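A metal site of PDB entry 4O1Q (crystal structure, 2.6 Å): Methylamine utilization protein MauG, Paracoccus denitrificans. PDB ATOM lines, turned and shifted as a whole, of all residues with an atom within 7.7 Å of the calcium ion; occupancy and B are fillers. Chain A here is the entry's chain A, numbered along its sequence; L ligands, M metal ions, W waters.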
ATOM      1  N   ARG A  45       2.777 -30.650   6.917  1.00  0.00           N
ATOM      2  CA  ARG A  45       3.430 -29.685   6.028  1.00  0.00           C
ATOM      3  C   ARG A  45       3.624 -30.222   4.600  1.00  0.00           C
ATOM      4  O   ARG A  45       4.754 -30.347   4.123  1.00  0.00           O
ATOM      5  CB  ARG A  45       4.780 -29.270   6.623  1.00  0.00           C
ATOM      6  CG  ARG A  45       5.398 -28.047   5.960  1.00  0.00           C
ATOM      7  CD  ARG A  45       6.542 -27.496   6.793  1.00  0.00           C
ATOM      8  NE  ARG A  45       7.551 -26.812   5.994  1.00  0.00           N
ATOM      9  CZ  ARG A  45       7.383 -25.649   5.377  1.00  0.00           C
ATOM     10  NH1 ARG A  45       6.230 -24.992   5.430  1.00  0.00           N
ATOM     11  NH2 ARG A  45       8.387 -25.127   4.673  1.00  0.00           N
ATOM     12  N   THR A  48       6.611 -32.258   3.742  1.00  0.00           N
ATOM     13  CA  THR A  48       7.954 -31.652   3.735  1.00  0.00           C
ATOM     14  C   THR A  48       8.403 -31.391   5.182  1.00  0.00           C
ATOM     15  O   THR A  48       7.635 -31.549   6.124  1.00  0.00           O
ATOM     16  CB  THR A  48       7.992 -30.327   2.930  1.00  0.00           C
ATOM     17  OG1 THR A  48       7.225 -29.308   3.589  1.00  0.00           O
ATOM     18  CG2 THR A  48       7.457 -30.533   1.516  1.00  0.00           C
ATOM     19  N   LEU A  57      15.563 -24.217   6.596  1.00  0.00           N
ATOM     20  CA  LEU A  57      14.745 -25.311   6.108  1.00  0.00           C
ATOM     21  C   LEU A  57      15.216 -25.767   4.712  1.00  0.00           C
ATOM     22  O   LEU A  57      14.584 -26.617   4.090  1.00  0.00           O
ATOM     23  CB  LEU A  57      13.256 -24.911   6.077  1.00  0.00           C
ATOM     24  CG  LEU A  57      12.513 -24.967   7.409  1.00  0.00           C
ATOM     25  CD1 LEU A  57      13.209 -24.171   8.507  1.00  0.00           C
ATOM     26  CD2 LEU A  57      11.077 -24.458   7.232  1.00  0.00           C
ATOM     27  N   ALA A  58      16.324 -25.195   4.229  1.00  0.00           N
ATOM     28  CA  ALA A  58      16.853 -25.522   2.900  1.00  0.00           C
ATOM     29  C   ALA A  58      17.194 -27.001   2.781  1.00  0.00           C
ATOM     30  O   ALA A  58      16.968 -27.600   1.741  1.00  0.00           O
ATOM     31  CB  ALA A  58      18.085 -24.680   2.588  1.00  0.00           C
ATOM     32  N   ASN A  72      16.903 -29.729  -1.032  1.00  0.00           N
ATOM     33  CA  ASN A  72      15.684 -29.476  -0.283  1.00  0.00           C
ATOM     34  C   ASN A  72      14.701 -30.641  -0.409  1.00  0.00           C
ATOM     35  O   ASN A  72      14.556 -31.238  -1.480  1.00  0.00           O
ATOM     36  CB  ASN A  72      15.029 -28.180  -0.776  1.00  0.00           C
ATOM     37  CG  ASN A  72      13.716 -27.894  -0.074  1.00  0.00           C
ATOM     38  OD1 ASN A  72      12.648 -27.922  -0.692  1.00  0.00           O
ATOM     39  ND2 ASN A  72      13.788 -27.614   1.228  1.00  0.00           N
ATOM     40  N   THR A  73      14.013 -30.934   0.691  1.00  0.00           N
ATOM     41  CA  THR A  73      13.051 -32.016   0.742  1.00  0.00           C
ATOM     42  C   THR A  73      11.768 -31.607   0.014  1.00  0.00           C
ATOM     43  O   THR A  73      11.145 -30.607   0.367  1.00  0.00           O
ATOM     44  CB  THR A  73      12.740 -32.409   2.203  1.00  0.00           C
ATOM     45  OG1 THR A  73      13.962 -32.530   2.936  1.00  0.00           O
ATOM     46  CG2 THR A  73      11.994 -33.722   2.274  1.00  0.00           C
ATOM     47  N   PRO A  74      11.376 -32.367  -1.028  1.00  0.00           N
ATOM     48  CA  PRO A  74      10.195 -32.032  -1.811  1.00  0.00           C
ATOM     49  C   PRO A  74       8.922 -32.647  -1.246  1.00  0.00           C
ATOM     50  O   PRO A  74       8.984 -33.651  -0.539  1.00  0.00           O
ATOM     51  CB  PRO A  74      10.512 -32.656  -3.174  1.00  0.00           C
ATOM     52  CG  PRO A  74      11.295 -33.870  -2.832  1.00  0.00           C
ATOM     53  CD  PRO A  74      12.082 -33.533  -1.581  1.00  0.00           C
ATOM     54  N   THR A  75       7.782 -32.062  -1.579  1.00  0.00           N
ATOM     55  CA  THR A  75       6.495 -32.697  -1.305  1.00  0.00           C
ATOM     56  C   THR A  75       6.472 -34.117  -1.863  1.00  0.00           C
ATOM     57  O   THR A  75       7.120 -34.411  -2.867  1.00  0.00           O
ATOM     58  CB  THR A  75       5.328 -31.881  -1.904  1.00  0.00           C
ATOM     59  OG1 THR A  75       4.083 -32.424  -1.456  1.00  0.00           O
ATOM     60  CG2 THR A  75       5.360 -31.877  -3.430  1.00  0.00           C
ATOM     61  N   TRP A  99      15.156 -34.615  -7.170  1.00  0.00           N
ATOM     62  CA  TRP A  99      15.416 -33.428  -8.000  1.00  0.00           C
ATOM     63  C   TRP A  99      16.259 -33.705  -9.236  1.00  0.00           C
ATOM     64  O   TRP A  99      16.164 -32.977 -10.223  1.00  0.00           O
ATOM     65  CB  TRP A  99      16.114 -32.344  -7.171  1.00  0.00           C
ATOM     66  CG  TRP A  99      15.226 -31.707  -6.163  1.00  0.00           C
ATOM     67  CD1 TRP A  99      15.181 -31.985  -4.835  1.00  0.00           C
ATOM     68  CD2 TRP A  99      14.264 -30.686  -6.407  1.00  0.00           C
ATOM     69  NE1 TRP A  99      14.255 -31.192  -4.224  1.00  0.00           N
ATOM     70  CE2 TRP A  99      13.665 -30.382  -5.161  1.00  0.00           C
ATOM     71  CE3 TRP A  99      13.846 -29.988  -7.537  1.00  0.00           C
ATOM     72  CZ2 TRP A  99      12.677 -29.412  -5.023  1.00  0.00           C
ATOM     73  CZ3 TRP A  99      12.858 -29.018  -7.399  1.00  0.00           C
ATOM     74  CH2 TRP A  99      12.283 -28.743  -6.156  1.00  0.00           C
ATOM     75  N   ASN A 277       0.634 -27.571  -4.244  1.00  0.00           N
ATOM     76  CA  ASN A 277       1.063 -27.325  -2.874  1.00  0.00           C
ATOM     77  C   ASN A 277       2.317 -26.454  -2.724  1.00  0.00           C
ATOM     78  O   ASN A 277       2.807 -26.241  -1.614  1.00  0.00           O
ATOM     79  CB  ASN A 277       1.225 -28.656  -2.116  1.00  0.00           C
ATOM     80  CG  ASN A 277      -0.104 -29.291  -1.764  1.00  0.00           C
ATOM     81  OD1 ASN A 277      -1.060 -28.590  -1.412  1.00  0.00           O
ATOM     82  ND2 ASN A 277      -0.176 -30.610  -1.848  1.00  0.00           N
ATOM     83  N   VAL A 278       2.784 -25.886  -3.838  1.00  0.00           N
ATOM     84  CA  VAL A 278       4.033 -25.136  -3.838  1.00  0.00           C
ATOM     85  C   VAL A 278       4.014 -23.991  -2.824  1.00  0.00           C
ATOM     86  O   VAL A 278       5.020 -23.694  -2.190  1.00  0.00           O
ATOM     87  CB  VAL A 278       4.365 -24.583  -5.255  1.00  0.00           C
ATOM     88  CG1 VAL A 278       3.453 -23.430  -5.644  1.00  0.00           C
ATOM     89  CG2 VAL A 278       5.828 -24.167  -5.322  1.00  0.00           C
ATOM     90  N   VAL A 280       2.968 -23.818   0.104  1.00  0.00           N
ATOM     91  CA  VAL A 280       3.208 -24.248   1.485  1.00  0.00           C
ATOM     92  C   VAL A 280       4.414 -25.186   1.655  1.00  0.00           C
ATOM     93  O   VAL A 280       4.487 -25.922   2.644  1.00  0.00           O
ATOM     94  CB  VAL A 280       1.941 -24.908   2.082  1.00  0.00           C
ATOM     95  CG1 VAL A 280       0.750 -23.958   1.974  1.00  0.00           C
ATOM     96  CG2 VAL A 280       1.613 -26.234   1.400  1.00  0.00           C
ATOM     97  N   THR A 281       5.365 -25.175   0.724  1.00  0.00           N
ATOM     98  CA  THR A 281       6.524 -26.077   0.785  1.00  0.00           C
ATOM     99  C   THR A 281       7.861 -25.351   0.575  1.00  0.00           C
ATOM    100  O   THR A 281       8.762 -25.878  -0.077  1.00  0.00           O
ATOM    101  CB  THR A 281       6.446 -27.201  -0.260  1.00  0.00           C
ATOM    102  OG1 THR A 281       6.480 -26.640  -1.575  1.00  0.00           O
ATOM    103  CG2 THR A 281       5.191 -28.022  -0.062  1.00  0.00           C
ATOM    104  N   GLY A 282       7.980 -24.152   1.134  1.00  0.00           N
ATOM    105  CA  GLY A 282       9.243 -23.432   1.091  1.00  0.00           C
ATOM    106  C   GLY A 282      10.286 -24.132   1.932  1.00  0.00           C
ATOM    107  O   GLY A 282       9.951 -25.001   2.736  1.00  0.00           O
ATOM    108  N   PRO A 283      11.583 -23.801   1.731  1.00  0.00           N
ATOM    109  CA  PRO A 283      12.102 -22.935   0.666  1.00  0.00           C
ATOM    110  C   PRO A 283      12.093 -23.635  -0.698  1.00  0.00           C
ATOM    111  O   PRO A 283      11.632 -24.776  -0.803  1.00  0.00           O
ATOM    112  CB  PRO A 283      13.519 -22.597   1.145  1.00  0.00           C
ATOM    113  CG  PRO A 283      13.904 -23.729   2.032  1.00  0.00           C
ATOM    114  CD  PRO A 283      12.634 -24.209   2.670  1.00  0.00           C
ATOM    115  N   TYR A 284      12.615 -22.965  -1.727  1.00  0.00           N
ATOM    116  CA  TYR A 284      12.352 -23.362  -3.105  1.00  0.00           C
ATOM    117  C   TYR A 284      13.579 -23.717  -3.937  1.00  0.00           C
ATOM    118  O   TYR A 284      14.710 -23.386  -3.588  1.00  0.00           O
ATOM    119  CB  TYR A 284      11.526 -22.279  -3.800  1.00  0.00           C
ATOM    120  CG  TYR A 284      10.200 -22.087  -3.107  1.00  0.00           C
ATOM    121  CD1 TYR A 284       9.162 -22.975  -3.321  1.00  0.00           C
ATOM    122  CD2 TYR A 284      10.008 -21.049  -2.195  1.00  0.00           C
ATOM    123  CE1 TYR A 284       7.946 -22.820  -2.680  1.00  0.00           C
ATOM    124  CE2 TYR A 284       8.799 -20.886  -1.546  1.00  0.00           C
ATOM    125  CZ  TYR A 284       7.778 -21.778  -1.785  1.00  0.00           C
ATOM    126  OH  TYR A 284       6.581 -21.622  -1.139  1.00  0.00           O
ATOM    127  N   MET A 285      13.313 -24.408  -5.039  1.00  0.00           N
ATOM    128  CA  MET A 285      14.337 -24.981  -5.910  1.00  0.00           C
ATOM    129  C   MET A 285      15.086 -26.111  -5.228  1.00  0.00           C
ATOM    130  O   MET A 285      14.926 -26.348  -4.022  1.00  0.00           O
ATOM    131  CB  MET A 285      15.324 -23.917  -6.405  1.00  0.00           C
ATOM    132  CG  MET A 285      14.677 -22.654  -6.957  1.00  0.00           C
ATOM    133  SD  MET A 285      13.503 -23.021  -8.265  1.00  0.00           S
ATOM    134  CE  MET A 285      13.334 -21.423  -9.059  1.00  0.00           C
ATOM    135  N   HIS A 286      15.898 -26.801  -6.017  1.00  0.00           N
ATOM    136  CA  HIS A 286      16.557 -28.038  -5.594  1.00  0.00           C
ATOM    137  C   HIS A 286      17.383 -27.843  -4.336  1.00  0.00           C
ATOM    138  O   HIS A 286      17.375 -28.691  -3.445  1.00  0.00           O
ATOM    139  CB  HIS A 286      17.425 -28.614  -6.738  1.00  0.00           C
ATOM    140  CG  HIS A 286      18.647 -27.792  -7.042  1.00  0.00           C
ATOM    141  ND1 HIS A 286      18.629 -26.734  -7.926  1.00  0.00           N
ATOM    142  CD2 HIS A 286      19.902 -27.859  -6.564  1.00  0.00           C
ATOM    143  CE1 HIS A 286      19.831 -26.182  -7.978  1.00  0.00           C
ATOM    144  NE2 HIS A 286      20.630 -26.853  -7.157  1.00  0.00           N
ATOM    145  N   GLY A 288      17.042 -25.333  -2.155  1.00  0.00           N
ATOM    146  CA  GLY A 288      16.287 -24.665  -1.108  1.00  0.00           C
ATOM    147  C   GLY A 288      16.807 -23.267  -0.817  1.00  0.00           C
ATOM    148  O   GLY A 288      16.819 -22.837   0.329  1.00  0.00           O
ATOM    149  N   PHE A 290      15.716 -20.213  -2.110  1.00  0.00           N
ATOM    150  CA  PHE A 290      14.721 -19.149  -2.006  1.00  0.00           C
ATOM    151  C   PHE A 290      13.698 -19.471  -0.926  1.00  0.00           C
ATOM    152  O   PHE A 290      12.960 -20.437  -1.043  1.00  0.00           O
ATOM    153  CB  PHE A 290      14.004 -18.911  -3.343  1.00  0.00           C
ATOM    154  CG  PHE A 290      14.935 -18.721  -4.513  1.00  0.00           C
ATOM    155  CD1 PHE A 290      16.040 -17.898  -4.418  1.00  0.00           C
ATOM    156  CD2 PHE A 290      14.663 -19.339  -5.727  1.00  0.00           C
ATOM    157  CE1 PHE A 290      16.887 -17.723  -5.504  1.00  0.00           C
ATOM    158  CE2 PHE A 290      15.501 -19.165  -6.816  1.00  0.00           C
ATOM    159  CZ  PHE A 290      16.621 -18.352  -6.699  1.00  0.00           C
HETATM  160 FE1  LIG L   1       9.720 -22.885 -12.950  1.00  0.00          FE
HETATM  161  C1  LIG L   1      11.138 -24.405 -10.201  1.00  0.00           C
HETATM  162  C2  LIG L   1       7.387 -21.288 -10.974  1.00  0.00           C
HETATM  163  C3  LIG L   1       8.882 -20.909 -15.644  1.00  0.00           C
HETATM  164  C4  LIG L   1      11.456 -25.023 -15.044  1.00  0.00           C
HETATM  165  N1  LIG L   1       9.312 -22.869 -10.905  1.00  0.00           N
HETATM  166  C5  LIG L   1       9.996 -23.493  -9.939  1.00  0.00           C
HETATM  167  C6  LIG L   1       9.475 -23.274  -8.573  1.00  0.00           C
HETATM  168  C7  LIG L   1       8.348 -22.352  -8.800  1.00  0.00           C
HETATM  169  C8  LIG L   1       8.344 -22.173 -10.272  1.00  0.00           C
HETATM  170  C9  LIG L   1       7.434 -21.753  -7.762  1.00  0.00           C
HETATM  171  C10 LIG L   1       9.982 -23.836  -7.265  1.00  0.00           C
HETATM  172  C11 LIG L   1       8.884 -24.656  -6.570  1.00  0.00           C
HETATM  173  C12 LIG L   1       9.439 -25.796  -5.738  1.00  0.00           C
HETATM  174  O1  LIG L   1       8.701 -26.789  -5.575  1.00  0.00           O
HETATM  175  O2  LIG L   1      10.589 -25.697  -5.252  1.00  0.00           O
HETATM  176  N2  LIG L   1       8.342 -21.365 -13.266  1.00  0.00           N
HETATM  177  C13 LIG L   1       7.485 -20.844 -12.384  1.00  0.00           C
HETATM  178  C14 LIG L   1       6.658 -19.726 -12.929  1.00  0.00           C
HETATM  179  C15 LIG L   1       7.123 -19.626 -14.316  1.00  0.00           C
HETATM  180  C16 LIG L   1       8.169 -20.654 -14.383  1.00  0.00           C
HETATM  181  C17 LIG L   1       5.595 -18.920 -12.238  1.00  0.00           C
HETATM  182  C18 LIG L   1       6.704 -18.679 -15.418  1.00  0.00           C
HETATM  183  C19 LIG L   1       7.137 -17.292 -14.993  1.00  0.00           C
HETATM  184  N3  LIG L   1      10.085 -22.962 -15.010  1.00  0.00           N
HETATM  185  C20 LIG L   1       9.718 -22.076 -15.944  1.00  0.00           C
HETATM  186  C21 LIG L   1      10.122 -22.378 -17.319  1.00  0.00           C
HETATM  187  C22 LIG L   1      10.904 -23.605 -17.124  1.00  0.00           C
HETATM  188  C23 LIG L   1      10.787 -23.877 -15.684  1.00  0.00           C
HETATM  189  C24 LIG L   1       9.866 -21.627 -18.600  1.00  0.00           C
HETATM  190  C25 LIG L   1      11.556 -24.440 -18.177  1.00  0.00           C
HETATM  191  C26 LIG L   1      12.435 -23.603 -19.070  1.00  0.00           C
HETATM  192  N4  LIG L   1      11.063 -24.471 -12.676  1.00  0.00           N
HETATM  193  C27 LIG L   1      11.667 -25.213 -13.609  1.00  0.00           C
HETATM  194  C28 LIG L   1      12.618 -26.226 -13.087  1.00  0.00           C
HETATM  195  C29 LIG L   1      12.525 -26.038 -11.649  1.00  0.00           C
HETATM  196  C30 LIG L   1      11.560 -24.911 -11.519  1.00  0.00           C
HETATM  197  C31 LIG L   1      13.451 -27.227 -13.843  1.00  0.00           C
HETATM  198  C32 LIG L   1      13.264 -26.760 -10.553  1.00  0.00           C
HETATM  199  C33 LIG L   1      14.225 -25.724  -9.963  1.00  0.00           C
HETATM  200  C34 LIG L   1      15.642 -26.228  -9.873  1.00  0.00           C
HETATM  201  O3  LIG L   1      16.310 -26.343 -10.919  1.00  0.00           O
HETATM  202  O4  LIG L   1      16.084 -26.494  -8.741  1.00  0.00           O
HETATM  203 CA    CA M   1      10.440 -26.881  -1.247  1.00  0.00          CA
HETATM  204  O   HOH W   1       9.344 -29.012  -0.990  1.00  0.00           O
HETATM  205  O   HOH W   2      11.385 -27.033  -3.133  1.00  0.00           O
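O2 of the ligand is in hydrogen-bond range of N of Met 285, 3.0 Å away. An oxygen (O4) of the ligand sits at hydrogen-bond distance from the backbone NH (N) of His 286 (2.7 Å). ND1 of His 286 is in hydrogen-bond range of O4 of the ligand (2.7 Å).
The side-chain amide nitrogen (ND2) of Asn 72 sits close to the backbone carbonyl oxygen (O) of Ala 58, at 3.2 Å. The side-chain amide nitrogen (ND2) of Asn 72 sits at hydrogen-bond distance from the backbone carbonyl oxygen (O) of Leu 57, 3.1 Å away. The side-chain hydroxyl of Thr 281 lies within hydrogen-bond range of the backbone carbonyl oxygen of Val 278, at 3.3 Å. The indole nitrogen (NE1) of Trp 99 is in hydrogen-bond range of the backbone carbonyl oxygen (O) of Asn 72. The backbone carbonyl oxygen of His 286 is in hydrogen-bond range of the backbone NH of Asn 72 (2.7 Å).
The calcium ion is bound by water W2 (2.1 Å). O of Thr 281 is bound to the calcium ion. Water W1 is bound to the calcium ion (2.4 Å). The calcium ion is bound by the backbone carbonyl oxygen (O) of Pro 283. The side-chain amide oxygen (OD1) of Asn 72 is bound to the calcium ion, at 2.5 Å.
Along chain A the residues within 4 Å of the calcium ion span positions 72 to 283.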
